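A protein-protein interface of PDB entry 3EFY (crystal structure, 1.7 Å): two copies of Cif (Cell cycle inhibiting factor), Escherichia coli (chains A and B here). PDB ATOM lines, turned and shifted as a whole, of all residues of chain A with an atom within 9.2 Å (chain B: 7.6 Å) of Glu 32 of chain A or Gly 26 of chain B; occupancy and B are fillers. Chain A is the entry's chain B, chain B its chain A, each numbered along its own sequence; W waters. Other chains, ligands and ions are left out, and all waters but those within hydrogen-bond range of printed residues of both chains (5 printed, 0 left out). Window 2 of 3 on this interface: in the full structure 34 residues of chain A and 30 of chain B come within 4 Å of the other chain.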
ATOM      1  N   ASN A  15     -17.024   8.033  19.445  1.00  0.00           N
ATOM      2  CA  ASN A  15     -16.471   8.515  18.170  1.00  0.00           C
ATOM      3  C   ASN A  15     -14.962   8.704  18.203  1.00  0.00           C
ATOM      4  O   ASN A  15     -14.266   8.332  17.292  1.00  0.00           O
ATOM      5  CB  ASN A  15     -17.110   9.807  17.717  1.00  0.00           C
ATOM      6  CG  ASN A  15     -18.613   9.662  17.486  1.00  0.00           C
ATOM      7  OD1 ASN A  15     -19.134   8.554  17.368  1.00  0.00           O
ATOM      8  ND2 ASN A  15     -19.325  10.804  17.429  1.00  0.00           N
ATOM      9  N   SER A  28     -10.022   9.546   7.591  1.00  0.00           N
ATOM     10  CA  SER A  28     -10.450  10.028   8.895  1.00  0.00           C
ATOM     11  C   SER A  28     -11.875   9.611   9.138  1.00  0.00           C
ATOM     12  O   SER A  28     -12.812   9.983   8.382  1.00  0.00           O
ATOM     13  CB  SER A  28     -10.358  11.555   9.012  1.00  0.00           C
ATOM     14  OG  SER A  28      -9.028  11.913   8.859  1.00  0.00           O
ATOM     15  N   TYR A  29     -12.049   8.836  10.178  1.00  0.00           N
ATOM     16  CA  TYR A  29     -13.370   8.396  10.615  1.00  0.00           C
ATOM     17  C   TYR A  29     -14.260   9.582  11.005  1.00  0.00           C
ATOM     18  O   TYR A  29     -13.792  10.485  11.695  1.00  0.00           O
ATOM     19  CB  TYR A  29     -13.220   7.412  11.769  1.00  0.00           C
ATOM     20  CG  TYR A  29     -14.533   7.014  12.425  1.00  0.00           C
ATOM     21  CD1 TYR A  29     -15.256   5.932  11.972  1.00  0.00           C
ATOM     22  CD2 TYR A  29     -15.096   7.772  13.428  1.00  0.00           C
ATOM     23  CE1 TYR A  29     -16.448   5.558  12.578  1.00  0.00           C
ATOM     24  CE2 TYR A  29     -16.293   7.401  14.041  1.00  0.00           C
ATOM     25  CZ  TYR A  29     -16.984   6.324  13.575  1.00  0.00           C
ATOM     26  OH  TYR A  29     -18.206   5.977  14.172  1.00  0.00           O
ATOM     27  N   CYS A  30     -15.513   9.566  10.533  1.00  0.00           N
ATOM     28  CA  CYS A  30     -16.529  10.575  10.836  1.00  0.00           C
ATOM     29  C   CYS A  30     -17.864   9.850  11.024  1.00  0.00           C
ATOM     30  O   CYS A  30     -18.453   9.344  10.050  1.00  0.00           O
ATOM     31  CB  CYS A  30     -16.631  11.586   9.707  1.00  0.00           C
ATOM     32  SG  CYS A  30     -17.777  12.904  10.171  1.00  0.00           S
ATOM     33  N   PHE A  31     -18.301   9.726  12.270  1.00  0.00           N
ATOM     34  CA  PHE A  31     -19.460   8.944  12.645  1.00  0.00           C
ATOM     35  C   PHE A  31     -20.670   9.158  11.738  1.00  0.00           C
ATOM     36  O   PHE A  31     -21.282   8.191  11.283  1.00  0.00           O
ATOM     37  CB  PHE A  31     -19.824   9.193  14.113  1.00  0.00           C
ATOM     38  CG  PHE A  31     -21.165   8.670  14.507  1.00  0.00           C
ATOM     39  CD1 PHE A  31     -21.404   7.299  14.588  1.00  0.00           C
ATOM     40  CD2 PHE A  31     -22.204   9.553  14.760  1.00  0.00           C
ATOM     41  CE1 PHE A  31     -22.690   6.810  14.951  1.00  0.00           C
ATOM     42  CE2 PHE A  31     -23.441   9.093  15.125  1.00  0.00           C
ATOM     43  CZ  PHE A  31     -23.692   7.723  15.240  1.00  0.00           C
ATOM     44  N   GLU A  32     -21.013  10.421  11.498  1.00  0.00           N
ATOM     45  CA  GLU A  32     -22.222  10.736  10.725  1.00  0.00           C
ATOM     46  C   GLU A  32     -22.154  10.308   9.288  1.00  0.00           C
ATOM     47  O   GLU A  32     -23.190  10.261   8.631  1.00  0.00           O
ATOM     48  CB  GLU A  32     -22.466  12.244  10.717  1.00  0.00           C
ATOM     49  CG  GLU A  32     -22.885  12.750  12.007  1.00  0.00           C
ATOM     50  CD  GLU A  32     -23.370  14.189  11.943  1.00  0.00           C
ATOM     51  OE1 GLU A  32     -23.419  14.780  10.823  1.00  0.00           O
ATOM     52  OE2 GLU A  32     -23.680  14.709  13.036  1.00  0.00           O
ATOM     53  N   ASN A  33     -20.966  10.012   8.774  1.00  0.00           N
ATOM     54  CA  ASN A  33     -20.797   9.680   7.362  1.00  0.00           C
ATOM     55  C   ASN A  33     -20.599   8.197   7.085  1.00  0.00           C
ATOM     56  O   ASN A  33     -20.635   7.780   5.924  1.00  0.00           O
ATOM     57  CB  ASN A  33     -19.634  10.433   6.801  1.00  0.00           C
ATOM     58  CG  ASN A  33     -19.814  11.935   6.891  1.00  0.00           C
ATOM     59  OD1 ASN A  33     -20.925  12.427   7.175  1.00  0.00           O
ATOM     60  ND2 ASN A  33     -18.745  12.662   6.692  1.00  0.00           N
ATOM     61  N   GLU A  34     -20.366   7.385   8.107  1.00  0.00           N
ATOM     62  CA  GLU A  34     -20.029   6.000   7.875  1.00  0.00           C
ATOM     63  C   GLU A  34     -21.254   5.115   7.704  1.00  0.00           C
ATOM     64  O   GLU A  34     -22.367   5.443   8.134  1.00  0.00           O
ATOM     65  CB  GLU A  34     -19.244   5.442   9.041  1.00  0.00           C
ATOM     66  CG  GLU A  34     -17.980   6.149   9.396  1.00  0.00           C
ATOM     67  CD  GLU A  34     -16.994   6.379   8.309  1.00  0.00           C
ATOM     68  OE1 GLU A  34     -16.891   5.583   7.338  1.00  0.00           O
ATOM     69  OE2 GLU A  34     -16.254   7.398   8.462  1.00  0.00           O
ATOM     70  N   GLN A  35     -21.027   3.953   7.115  1.00  0.00           N
ATOM     71  CA  GLN A  35     -22.139   3.039   6.898  1.00  0.00           C
ATOM     72  C   GLN A  35     -22.587   2.354   8.180  1.00  0.00           C
ATOM     73  O   GLN A  35     -21.762   2.044   9.022  1.00  0.00           O
ATOM     74  CB  GLN A  35     -21.789   2.080   5.759  1.00  0.00           C
ATOM     75  CG  GLN A  35     -21.820   2.850   4.369  1.00  0.00           C
ATOM     76  CD  GLN A  35     -23.154   3.641   4.028  1.00  0.00           C
ATOM     77  OE1 GLN A  35     -23.212   4.899   4.090  1.00  0.00           O
ATOM     78  NE2 GLN A  35     -24.199   2.896   3.610  1.00  0.00           N
ATOM     79  N   THR A  36     -23.907   2.199   8.347  1.00  0.00           N
ATOM     80  CA  THR A  36     -24.472   1.541   9.522  1.00  0.00           C
ATOM     81  C   THR A  36     -25.091   0.209   9.193  1.00  0.00           C
ATOM     82  O   THR A  36     -25.493  -0.043   8.026  1.00  0.00           O
ATOM     83  CB  THR A  36     -25.504   2.415  10.170  1.00  0.00           C
ATOM     84  OG1 THR A  36     -26.640   2.502   9.305  1.00  0.00           O
ATOM     85  CG2 THR A  36     -24.908   3.800  10.407  1.00  0.00           C
ATOM     86  N   ARG A  58     -18.969  -0.117  16.925  1.00  0.00           N
ATOM     87  CA  ARG A  58     -19.550   1.038  17.590  1.00  0.00           C
ATOM     88  C   ARG A  58     -21.035   0.734  17.767  1.00  0.00           C
ATOM     89  O   ARG A  58     -21.726   0.439  16.767  1.00  0.00           O
ATOM     90  CB  ARG A  58     -19.361   2.332  16.828  1.00  0.00           C
ATOM     91  CG  ARG A  58     -19.828   3.525  17.681  1.00  0.00           C
ATOM     92  CD  ARG A  58     -19.941   4.718  16.799  1.00  0.00           C
ATOM     93  NE  ARG A  58     -20.271   5.944  17.465  1.00  0.00           N
ATOM     94  CZ  ARG A  58     -21.473   6.251  17.967  1.00  0.00           C
ATOM     95  NH1 ARG A  58     -22.478   5.379  17.912  1.00  0.00           N
ATOM     96  NH2 ARG A  58     -21.648   7.455  18.535  1.00  0.00           N
ATOM     97  N   GLN A 162     -21.855   0.170  13.782  1.00  0.00           N
ATOM     98  CA  GLN A 162     -20.834   0.343  12.749  1.00  0.00           C
ATOM     99  C   GLN A 162     -19.735  -0.643  13.080  1.00  0.00           C
ATOM    100  O   GLN A 162     -19.260  -0.706  14.243  1.00  0.00           O
ATOM    101  CB  GLN A 162     -20.296   1.763  12.651  1.00  0.00           C
ATOM    102  CG  GLN A 162     -21.332   2.822  12.341  1.00  0.00           C
ATOM    103  CD  GLN A 162     -20.778   4.198  12.264  1.00  0.00           C
ATOM    104  OE1 GLN A 162     -19.640   4.437  12.644  1.00  0.00           O
ATOM    105  NE2 GLN A 162     -21.605   5.139  11.832  1.00  0.00           N
ATOM    106  N   LEU B  22     -10.563  21.362  14.850  1.00  0.00           N
ATOM    107  CA  LEU B  22     -11.621  21.310  13.827  1.00  0.00           C
ATOM    108  C   LEU B  22     -12.632  20.192  13.902  1.00  0.00           C
ATOM    109  O   LEU B  22     -13.768  20.372  13.414  1.00  0.00           O
ATOM    110  CB  LEU B  22     -10.990  21.289  12.444  1.00  0.00           C
ATOM    111  CG  LEU B  22     -10.050  22.447  12.145  1.00  0.00           C
ATOM    112  CD1 LEU B  22      -9.312  22.299  10.775  1.00  0.00           C
ATOM    113  CD2 LEU B  22     -10.781  23.811  12.187  1.00  0.00           C
ATOM    114  N   ASP B  23     -12.278  19.056  14.489  1.00  0.00           N
ATOM    115  CA  ASP B  23     -13.178  17.912  14.443  1.00  0.00           C
ATOM    116  C   ASP B  23     -14.416  18.147  15.294  1.00  0.00           C
ATOM    117  O   ASP B  23     -14.350  18.659  16.405  1.00  0.00           O
ATOM    118  CB  ASP B  23     -12.490  16.645  14.871  1.00  0.00           C
ATOM    119  CG  ASP B  23     -11.538  16.076  13.805  1.00  0.00           C
ATOM    120  OD1 ASP B  23     -11.350  16.716  12.781  1.00  0.00           O
ATOM    121  OD2 ASP B  23     -10.974  14.993  14.051  1.00  0.00           O
ATOM    122  N   LYS B  24     -15.553  17.785  14.729  1.00  0.00           N
ATOM    123  CA  LYS B  24     -16.826  17.937  15.397  1.00  0.00           C
ATOM    124  C   LYS B  24     -17.816  16.987  14.786  1.00  0.00           C
ATOM    125  O   LYS B  24     -17.488  16.268  13.877  1.00  0.00           O
ATOM    126  CB  LYS B  24     -17.282  19.394  15.291  1.00  0.00           C
ATOM    127  CG  LYS B  24     -17.496  19.886  13.960  1.00  0.00           C
ATOM    128  CD  LYS B  24     -17.680  21.390  13.930  1.00  0.00           C
ATOM    129  CE  LYS B  24     -18.245  21.835  12.587  1.00  0.00           C
ATOM    130  NZ  LYS B  24     -17.398  21.658  11.342  1.00  0.00           N
ATOM    131  N   ASP B  25     -19.053  16.995  15.289  1.00  0.00           N
ATOM    132  CA  ASP B  25     -20.083  16.183  14.676  1.00  0.00           C
ATOM    133  C   ASP B  25     -20.219  16.562  13.215  1.00  0.00           C
ATOM    134  O   ASP B  25     -20.387  17.761  12.868  1.00  0.00           O
ATOM    135  CB  ASP B  25     -21.409  16.387  15.411  1.00  0.00           C
ATOM    136  CG  ASP B  25     -21.435  15.769  16.793  1.00  0.00           C
ATOM    137  OD1 ASP B  25     -20.668  14.817  17.127  1.00  0.00           O
ATOM    138  OD2 ASP B  25     -22.284  16.238  17.592  1.00  0.00           O
ATOM    139  N   GLY B  26     -20.076  15.582  12.326  1.00  0.00           N
ATOM    140  CA  GLY B  26     -20.177  15.851  10.891  1.00  0.00           C
ATOM    141  C   GLY B  26     -18.962  16.416  10.154  1.00  0.00           C
ATOM    142  O   GLY B  26     -19.005  16.626   8.955  1.00  0.00           O
ATOM    143  N   PHE B  27     -17.838  16.623  10.847  1.00  0.00           N
ATOM    144  CA  PHE B  27     -16.616  17.032  10.174  1.00  0.00           C
ATOM    145  C   PHE B  27     -15.415  16.369  10.830  1.00  0.00           C
ATOM    146  O   PHE B  27     -15.172  16.509  12.049  1.00  0.00           O
ATOM    147  CB  PHE B  27     -16.375  18.546  10.176  1.00  0.00           C
ATOM    148  CG  PHE B  27     -15.131  18.920   9.464  1.00  0.00           C
ATOM    149  CD1 PHE B  27     -15.078  18.890   8.075  1.00  0.00           C
ATOM    150  CD2 PHE B  27     -13.975  19.230  10.147  1.00  0.00           C
ATOM    151  CE1 PHE B  27     -13.910  19.200   7.394  1.00  0.00           C
ATOM    152  CE2 PHE B  27     -12.807  19.536   9.470  1.00  0.00           C
ATOM    153  CZ  PHE B  27     -12.769  19.517   8.075  1.00  0.00           C
ATOM    154  N   SER B  28     -14.661  15.655  10.006  1.00  0.00           N
ATOM    155  CA  SER B  28     -13.376  15.111  10.428  1.00  0.00           C
ATOM    156  C   SER B  28     -12.299  15.560   9.435  1.00  0.00           C
ATOM    157  O   SER B  28     -12.334  15.236   8.251  1.00  0.00           O
ATOM    158  CB  SER B  28     -13.382  13.576  10.515  1.00  0.00           C
ATOM    159  OG  SER B  28     -14.287  13.162  11.511  1.00  0.00           O
HETATM  160  O   HOH W   1     -18.506  15.445   6.712  1.00  0.00           O
HETATM  161  O   HOH W   2     -17.979  13.451  17.241  1.00  0.00           O
HETATM  162  O   HOH W   3     -21.174  12.649  19.518  1.00  0.00           O
HETATM  163  O   HOH W   4     -21.378  15.075   7.789  1.00  0.00           O
HETATM  164  O   HOH W   5     -19.981  12.690  13.220  1.00  0.00           O
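CB of Ser 28 of chain A touches CB of Ser 28 of chain B (3.9 Å).
C of Gly 26 of chain B touches SG of Cys 30 of chain A, 3.7 Å away.
Asp 25 of chain B touches Glu 32 of chain A.
Gly 26 of chain B touches Glu 32 of chain A.
Water W1 lies within hydrogen-bond range of O of Gly 26 of chain B (2.6 Å) and ND2 of Asn 33 of chain A (2.8 Å).
Water W4 lies within hydrogen-bond range of OD1 of Asn 33 of chain A (2.8 Å) and O of Gly 26 of chain B (3.1 Å).
Water W2 bridges the side-chain amide nitrogen of Asn 15 of chain A and the side-chain carboxylate of Asp 25 of chain B.
Water W5 lies within hydrogen-bond range of the backbone NH of Gly 26 of chain B (3.0 Å), the backbone NH of Glu 32 of chain A (3.0 Å) and the side-chain sulfur of Cys 30 of chain A (3.8 Å).
Water W3 lies within hydrogen-bond range of the side-chain carboxylate (OD1) of Asp 25 of chain B (3.3 Å) and the side-chain amide nitrogen (ND2) of Asn 15 of chain A (3.3 Å).
SG of Cys 30 of chain A lies within hydrogen-bond range of ND2 of Asn 33 of chain A (3.6 Å).
The backbone NH (N) of Cys 30 of chain A lies within hydrogen-bond range of the side-chain carboxylate (OE2) of Glu 34 of chain A, at 3.1 Å.
OH of Tyr 29 of chain A is in hydrogen-bond range of OE1 of Gln 162 of chain A, at 2.6 Å.
Ser 28 of chain B touches its own counterpart, Ser 28 of chain A.
Position printed for both chains: 28.
Of the 7 pairs that touch across the chains among the printed residues, 1 has its exchanged pair printed and touching as well.
Among the printed residues, no Asp or Glu carboxylate lies within 4 Å of a Lys or Arg side-chain nitrogen of the other chain.
Of chain B, only Asp 25 and Gly 26 come within 4 Å of Glu 32 of chain A.
Of chain A, only Cys 30 (3.7 Å) and Glu 32 (3.4 Å) come within 4 Å of Gly 26 of chain B.
Of the printed residues of chain B, Ser 28 of chain A touches Ser 28 (3.9 Å).
Of the printed residues of chain A, Ser 28 of chain B touches Ser 28, Tyr 29 and Cys 30.
Of the printed residues of chain B, Cys 30 of chain A touches Gly 26, Phe 27 and Ser 28.
Leu 22 of chain B touches none of the printed residues of chain A.
The nearest residue of chain B that does not touch Glu 32 of chain A is Phe 27 of chain B (5.9 Å).
The nearest residue of chain A that does not touch Gly 26 of chain B is Asn 33 of chain A (4.6 Å).
The nearest printed residue of chain B that does not touch Cys 30 of chain A is Lys 24 of chain B (5.0 Å).
The backbone NH (N) of Phe 27 of chain B is in hydrogen-bond range of the side-chain sulfur (SG) of Cys 30 of chain A.
OG of Ser 28 of chain B sits close to SG of Cys 30 of chain A (3.7 Å).
O of Tyr 29 of chain A sits at hydrogen-bond distance from OG of Ser 28 of chain B (2.7 Å).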
